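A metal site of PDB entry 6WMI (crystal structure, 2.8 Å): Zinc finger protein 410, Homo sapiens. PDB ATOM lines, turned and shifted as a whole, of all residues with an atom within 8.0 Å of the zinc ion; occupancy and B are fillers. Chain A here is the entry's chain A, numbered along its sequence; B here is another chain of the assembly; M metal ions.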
ATOM      1  N   MET A  69      13.418  -0.859 -26.008  1.00  0.00           N
ATOM      2  CA  MET A  69      12.827  -1.552 -27.152  1.00  0.00           C
ATOM      3  C   MET A  69      13.346  -2.984 -27.248  1.00  0.00           C
ATOM      4  O   MET A  69      14.533  -3.242 -27.049  1.00  0.00           O
ATOM      5  CB  MET A  69      13.137  -0.805 -28.437  1.00  0.00           C
ATOM      6  CG  MET A  69      12.402  -1.334 -29.654  1.00  0.00           C
ATOM      7  SD  MET A  69      12.928  -0.469 -31.135  1.00  0.00           S
ATOM      8  CE  MET A  69      14.444  -1.335 -31.525  1.00  0.00           C
ATOM      9  N   CYS A  70      12.442  -3.907 -27.573  1.00  0.00           N
ATOM     10  CA  CYS A  70      12.836  -5.265 -27.903  1.00  0.00           C
ATOM     11  C   CYS A  70      13.431  -5.290 -29.308  1.00  0.00           C
ATOM     12  O   CYS A  70      12.817  -4.780 -30.254  1.00  0.00           O
ATOM     13  CB  CYS A  70      11.637  -6.206 -27.810  1.00  0.00           C
ATOM     14  SG  CYS A  70      12.001  -7.943 -28.101  1.00  0.00           S
ATOM     15  N   HIS A  71      14.622  -5.880 -29.449  1.00  0.00           N
ATOM     16  CA  HIS A  71      15.298  -5.968 -30.740  1.00  0.00           C
ATOM     17  C   HIS A  71      15.100  -7.318 -31.410  1.00  0.00           C
ATOM     18  O   HIS A  71      15.840  -7.646 -32.349  1.00  0.00           O
ATOM     19  CB  HIS A  71      16.783  -5.682 -30.577  1.00  0.00           C
ATOM     20  CG  HIS A  71      17.094  -4.255 -30.251  1.00  0.00           C
ATOM     21  ND1 HIS A  71      17.234  -3.795 -28.965  1.00  0.00           N
ATOM     22  CD2 HIS A  71      17.292  -3.179 -31.058  1.00  0.00           C
ATOM     23  CE1 HIS A  71      17.500  -2.507 -28.971  1.00  0.00           C
ATOM     24  NE2 HIS A  71      17.543  -2.107 -30.232  1.00  0.00           N
ATOM     25  N   GLU A  72      14.150  -8.123 -30.940  1.00  0.00           N
ATOM     26  CA  GLU A  72      13.778  -9.322 -31.659  1.00  0.00           C
ATOM     27  C   GLU A  72      13.231  -8.954 -33.031  1.00  0.00           C
ATOM     28  O   GLU A  72      12.450  -8.004 -33.162  1.00  0.00           O
ATOM     29  CB  GLU A  72      12.737 -10.121 -30.859  1.00  0.00           C
ATOM     30  CG  GLU A  72      12.359 -11.468 -31.440  1.00  0.00           C
ATOM     31  CD  GLU A  72      13.461 -12.505 -31.323  1.00  0.00           C
ATOM     32  OE1 GLU A  72      14.263 -12.413 -30.359  1.00  0.00           O
ATOM     33  OE2 GLU A  72      13.526 -13.399 -32.186  1.00  0.00           O
ATOM     34  N   SER A  73      13.656  -9.689 -34.048  1.00  0.00           N
ATOM     35  CA  SER A  73      13.162  -9.418 -35.390  1.00  0.00           C
ATOM     36  C   SER A  73      11.657  -9.615 -35.429  1.00  0.00           C
ATOM     37  O   SER A  73      11.136 -10.661 -35.030  1.00  0.00           O
ATOM     38  CB  SER A  73      13.839 -10.343 -36.399  1.00  0.00           C
ATOM     39  OG  SER A  73      13.374 -10.056 -37.704  1.00  0.00           O
ATOM     40  N   GLY A  74      10.952  -8.594 -35.922  1.00  0.00           N
ATOM     41  CA  GLY A  74       9.511  -8.631 -36.014  1.00  0.00           C
ATOM     42  C   GLY A  74       8.776  -8.128 -34.793  1.00  0.00           C
ATOM     43  O   GLY A  74       7.565  -7.902 -34.866  1.00  0.00           O
ATOM     44  N   CYS A  75       9.470  -7.935 -33.658  1.00  0.00           N
ATOM     45  CA  CYS A  75       8.780  -7.502 -32.439  1.00  0.00           C
ATOM     46  C   CYS A  75       8.818  -5.985 -32.282  1.00  0.00           C
ATOM     47  O   CYS A  75       7.795  -5.319 -32.453  1.00  0.00           O
ATOM     48  CB  CYS A  75       9.410  -8.195 -31.230  1.00  0.00           C
ATOM     49  SG  CYS A  75       8.592  -7.857 -29.663  1.00  0.00           S
ATOM     50  N   GLY A  76      10.006  -5.424 -32.048  1.00  0.00           N
ATOM     51  CA  GLY A  76      10.161  -4.007 -31.801  1.00  0.00           C
ATOM     52  C   GLY A  76       9.194  -3.367 -30.814  1.00  0.00           C
ATOM     53  O   GLY A  76       8.850  -2.189 -30.969  1.00  0.00           O
ATOM     54  N   LYS A  77       8.732  -4.098 -29.804  1.00  0.00           N
ATOM     55  CA  LYS A  77       7.867  -3.487 -28.804  1.00  0.00           C
ATOM     56  C   LYS A  77       8.683  -2.607 -27.860  1.00  0.00           C
ATOM     57  O   LYS A  77       9.873  -2.841 -27.629  1.00  0.00           O
ATOM     58  CB  LYS A  77       7.118  -4.556 -27.989  1.00  0.00           C
ATOM     59  CG  LYS A  77       6.015  -5.261 -28.763  1.00  0.00           C
ATOM     60  CD  LYS A  77       5.086  -6.021 -27.826  1.00  0.00           C
ATOM     61  CE  LYS A  77       4.184  -6.997 -28.590  1.00  0.00           C
ATOM     62  NZ  LYS A  77       3.216  -6.309 -29.499  1.00  0.00           N
ATOM     63  N   GLN A  78       8.032  -1.572 -27.325  1.00  0.00           N
ATOM     64  CA  GLN A  78       8.696  -0.574 -26.494  1.00  0.00           C
ATOM     65  C   GLN A  78       8.073  -0.546 -25.101  1.00  0.00           C
ATOM     66  O   GLN A  78       6.856  -0.649 -24.949  1.00  0.00           O
ATOM     67  CB  GLN A  78       8.617   0.814 -27.134  1.00  0.00           C
ATOM     68  CG  GLN A  78       9.332   0.926 -28.479  1.00  0.00           C
ATOM     69  CD  GLN A  78       9.279   2.324 -29.066  1.00  0.00           C
ATOM     70  OE1 GLN A  78       8.378   2.643 -29.866  1.00  0.00           O
ATOM     71  NE2 GLN A  78      10.219   3.163 -28.680  1.00  0.00           N
ATOM     72  N   PHE A  79       8.926  -0.391 -24.089  1.00  0.00           N
ATOM     73  CA  PHE A  79       8.519  -0.486 -22.698  1.00  0.00           C
ATOM     74  C   PHE A  79       9.033   0.714 -21.918  1.00  0.00           C
ATOM     75  O   PHE A  79      10.036   1.327 -22.284  1.00  0.00           O
ATOM     76  CB  PHE A  79       9.020  -1.794 -22.069  1.00  0.00           C
ATOM     77  CG  PHE A  79       8.489  -3.029 -22.733  1.00  0.00           C
ATOM     78  CD1 PHE A  79       9.110  -3.552 -23.852  1.00  0.00           C
ATOM     79  CD2 PHE A  79       7.360  -3.663 -22.238  1.00  0.00           C
ATOM     80  CE1 PHE A  79       8.615  -4.683 -24.473  1.00  0.00           C
ATOM     81  CE2 PHE A  79       6.857  -4.790 -22.848  1.00  0.00           C
ATOM     82  CZ  PHE A  79       7.486  -5.311 -23.970  1.00  0.00           C
ATOM     83  N   LEU A  85      10.967  -4.781 -20.027  1.00  0.00           N
ATOM     84  CA  LEU A  85      11.530  -5.365 -21.245  1.00  0.00           C
ATOM     85  C   LEU A  85      12.243  -6.673 -20.938  1.00  0.00           C
ATOM     86  O   LEU A  85      12.100  -7.653 -21.680  1.00  0.00           O
ATOM     87  CB  LEU A  85      12.491  -4.372 -21.896  1.00  0.00           C
ATOM     88  CG  LEU A  85      13.371  -4.893 -23.029  1.00  0.00           C
ATOM     89  CD1 LEU A  85      12.531  -5.427 -24.170  1.00  0.00           C
ATOM     90  CD2 LEU A  85      14.295  -3.804 -23.534  1.00  0.00           C
ATOM     91  N   HIS A  88       9.716  -9.256 -20.726  1.00  0.00           N
ATOM     92  CA  HIS A  88       9.135  -9.534 -22.034  1.00  0.00           C
ATOM     93  C   HIS A  88      10.030 -10.445 -22.873  1.00  0.00           C
ATOM     94  O   HIS A  88       9.548 -11.409 -23.495  1.00  0.00           O
ATOM     95  CB  HIS A  88       8.855  -8.231 -22.768  1.00  0.00           C
ATOM     96  CG  HIS A  88       8.728  -8.394 -24.254  1.00  0.00           C
ATOM     97  ND1 HIS A  88       7.570  -8.826 -24.864  1.00  0.00           N
ATOM     98  CD2 HIS A  88       9.625  -8.180 -25.253  1.00  0.00           C
ATOM     99  CE1 HIS A  88       7.755  -8.879 -26.174  1.00  0.00           C
ATOM    100  NE2 HIS A  88       8.988  -8.491 -26.430  1.00  0.00           N
ATOM    101  N   ARG A  89      11.341 -10.176 -22.882  1.00  0.00           N
ATOM    102  CA  ARG A  89      12.269 -10.946 -23.718  1.00  0.00           C
ATOM    103  C   ARG A  89      12.166 -12.445 -23.492  1.00  0.00           C
ATOM    104  O   ARG A  89      12.576 -13.221 -24.364  1.00  0.00           O
ATOM    105  CB  ARG A  89      13.709 -10.509 -23.477  1.00  0.00           C
ATOM    106  CG  ARG A  89      14.077  -9.201 -24.147  1.00  0.00           C
ATOM    107  CD  ARG A  89      15.585  -8.950 -24.111  1.00  0.00           C
ATOM    108  NE  ARG A  89      16.344 -10.129 -24.496  1.00  0.00           N
ATOM    109  CZ  ARG A  89      16.458 -10.578 -25.738  1.00  0.00           C
ATOM    110  NH1 ARG A  89      15.840  -9.952 -26.746  1.00  0.00           N
ATOM    111  NH2 ARG A  89      17.169 -11.671 -25.983  1.00  0.00           N
ATOM    112  N   ARG A  90      11.632 -12.879 -22.348  1.00  0.00           N
ATOM    113  CA  ARG A  90      11.559 -14.308 -22.066  1.00  0.00           C
ATOM    114  C   ARG A  90      10.563 -15.028 -22.964  1.00  0.00           C
ATOM    115  O   ARG A  90      10.623 -16.260 -23.081  1.00  0.00           O
ATOM    116  CB  ARG A  90      11.209 -14.531 -20.596  1.00  0.00           C
ATOM    117  CG  ARG A  90      12.203 -13.865 -19.657  1.00  0.00           C
ATOM    118  CD  ARG A  90      12.219 -14.496 -18.276  1.00  0.00           C
ATOM    119  NE  ARG A  90      13.363 -14.043 -17.491  1.00  0.00           N
ATOM    120  CZ  ARG A  90      13.323 -13.036 -16.640  1.00  0.00           C
ATOM    121  NH1 ARG A  90      12.198 -12.364 -16.455  1.00  0.00           N
ATOM    122  NH2 ARG A  90      14.424 -12.674 -15.971  1.00  0.00           N
ATOM    123  N   ILE A  91       9.656 -14.307 -23.626  1.00  0.00           N
ATOM    124  CA  ILE A  91       8.782 -14.978 -24.572  1.00  0.00           C
ATOM    125  C   ILE A  91       9.532 -15.366 -25.832  1.00  0.00           C
ATOM    126  O   ILE A  91       9.117 -16.287 -26.542  1.00  0.00           O
ATOM    127  CB  ILE A  91       7.541 -14.131 -24.923  1.00  0.00           C
ATOM    128  CG1 ILE A  91       7.888 -13.018 -25.910  1.00  0.00           C
ATOM    129  CG2 ILE A  91       6.922 -13.538 -23.668  1.00  0.00           C
ATOM    130  CD1 ILE A  91       6.723 -12.129 -26.224  1.00  0.00           C
ATOM    131  N   HIS A  92      10.653 -14.707 -26.131  1.00  0.00           N
ATOM    132  CA  HIS A  92      11.489 -15.091 -27.262  1.00  0.00           C
ATOM    133  C   HIS A  92      12.602 -16.053 -26.876  1.00  0.00           C
ATOM    134  O   HIS A  92      13.062 -16.827 -27.729  1.00  0.00           O
ATOM    135  CB  HIS A  92      12.116 -13.867 -27.932  1.00  0.00           C
ATOM    136  CG  HIS A  92      11.167 -12.745 -28.202  1.00  0.00           C
ATOM    137  ND1 HIS A  92      10.090 -12.862 -29.058  1.00  0.00           N
ATOM    138  CD2 HIS A  92      11.150 -11.466 -27.747  1.00  0.00           C
ATOM    139  CE1 HIS A  92       9.448 -11.707 -29.106  1.00  0.00           C
ATOM    140  NE2 HIS A  92      10.073 -10.844 -28.320  1.00  0.00           N
ATOM    141  P    DC B   7       3.844  -8.763 -23.879  1.00  0.00           P
ATOM    142  OP1  DC B   7       3.674  -8.428 -25.311  1.00  0.00           O
ATOM    143  OP2  DC B   7       5.193  -9.015 -23.322  1.00  0.00           O
ATOM    144  O5'  DC B   7       3.174  -7.588 -23.034  1.00  0.00           O
ATOM    145  C5'  DC B   7       1.854  -7.176 -23.350  1.00  0.00           C
ATOM    146  C4'  DC B   7       1.335  -6.201 -22.317  1.00  0.00           C
ATOM    147  O4'  DC B   7       1.220  -6.869 -21.035  1.00  0.00           O
ATOM    148  C3'  DC B   7       2.216  -4.973 -22.095  1.00  0.00           C
ATOM    149  O3'  DC B   7       1.443  -3.795 -22.311  1.00  0.00           O
ATOM    150  C2'  DC B   7       2.661  -5.103 -20.630  1.00  0.00           C
ATOM    151  C1'  DC B   7       1.556  -5.951 -20.038  1.00  0.00           C
ATOM    152  N1   DC B   7       1.965  -6.714 -18.832  1.00  0.00           N
ATOM    153  C2   DC B   7       1.398  -6.396 -17.587  1.00  0.00           C
ATOM    154  O2   DC B   7       0.572  -5.482 -17.524  1.00  0.00           O
ATOM    155  N3   DC B   7       1.775  -7.109 -16.492  1.00  0.00           N
ATOM    156  C4   DC B   7       2.670  -8.091 -16.611  1.00  0.00           C
ATOM    157  N4   DC B   7       3.013  -8.768 -15.515  1.00  0.00           N
ATOM    158  C5   DC B   7       3.249  -8.426 -17.869  1.00  0.00           C
ATOM    159  C6   DC B   7       2.867  -7.718 -18.948  1.00  0.00           C
HETATM  160 ZN    ZN M   1       9.879  -8.827 -28.206  1.00  0.00          ZN
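Within 4 Å of the zinc ion: Cys 70, Cys 75, His 88 and His 92.
OP2 of DC 7 of chain B lies within hydrogen-bond range of a ring nitrogen (ND1) of His 88 (2.8 Å).
The side-chain sulfur (SG) of Cys 70 sits close to the backbone NH (N) of Glu 72 (3.6 Å).
N of Cys 70 sits at hydrogen-bond distance from O of Lys 77, 2.8 Å away.
N of Lys 77 sits close to SG of Cys 75, 3.8 Å away.
The backbone carbonyl oxygen (O) of Cys 70 sits close to the backbone NH (N) of Gly 76 (3.4 Å).
The zinc ion is bound by NE2 of His 88, NE2 of His 92, SG of Cys 75 and SG of Cys 70.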
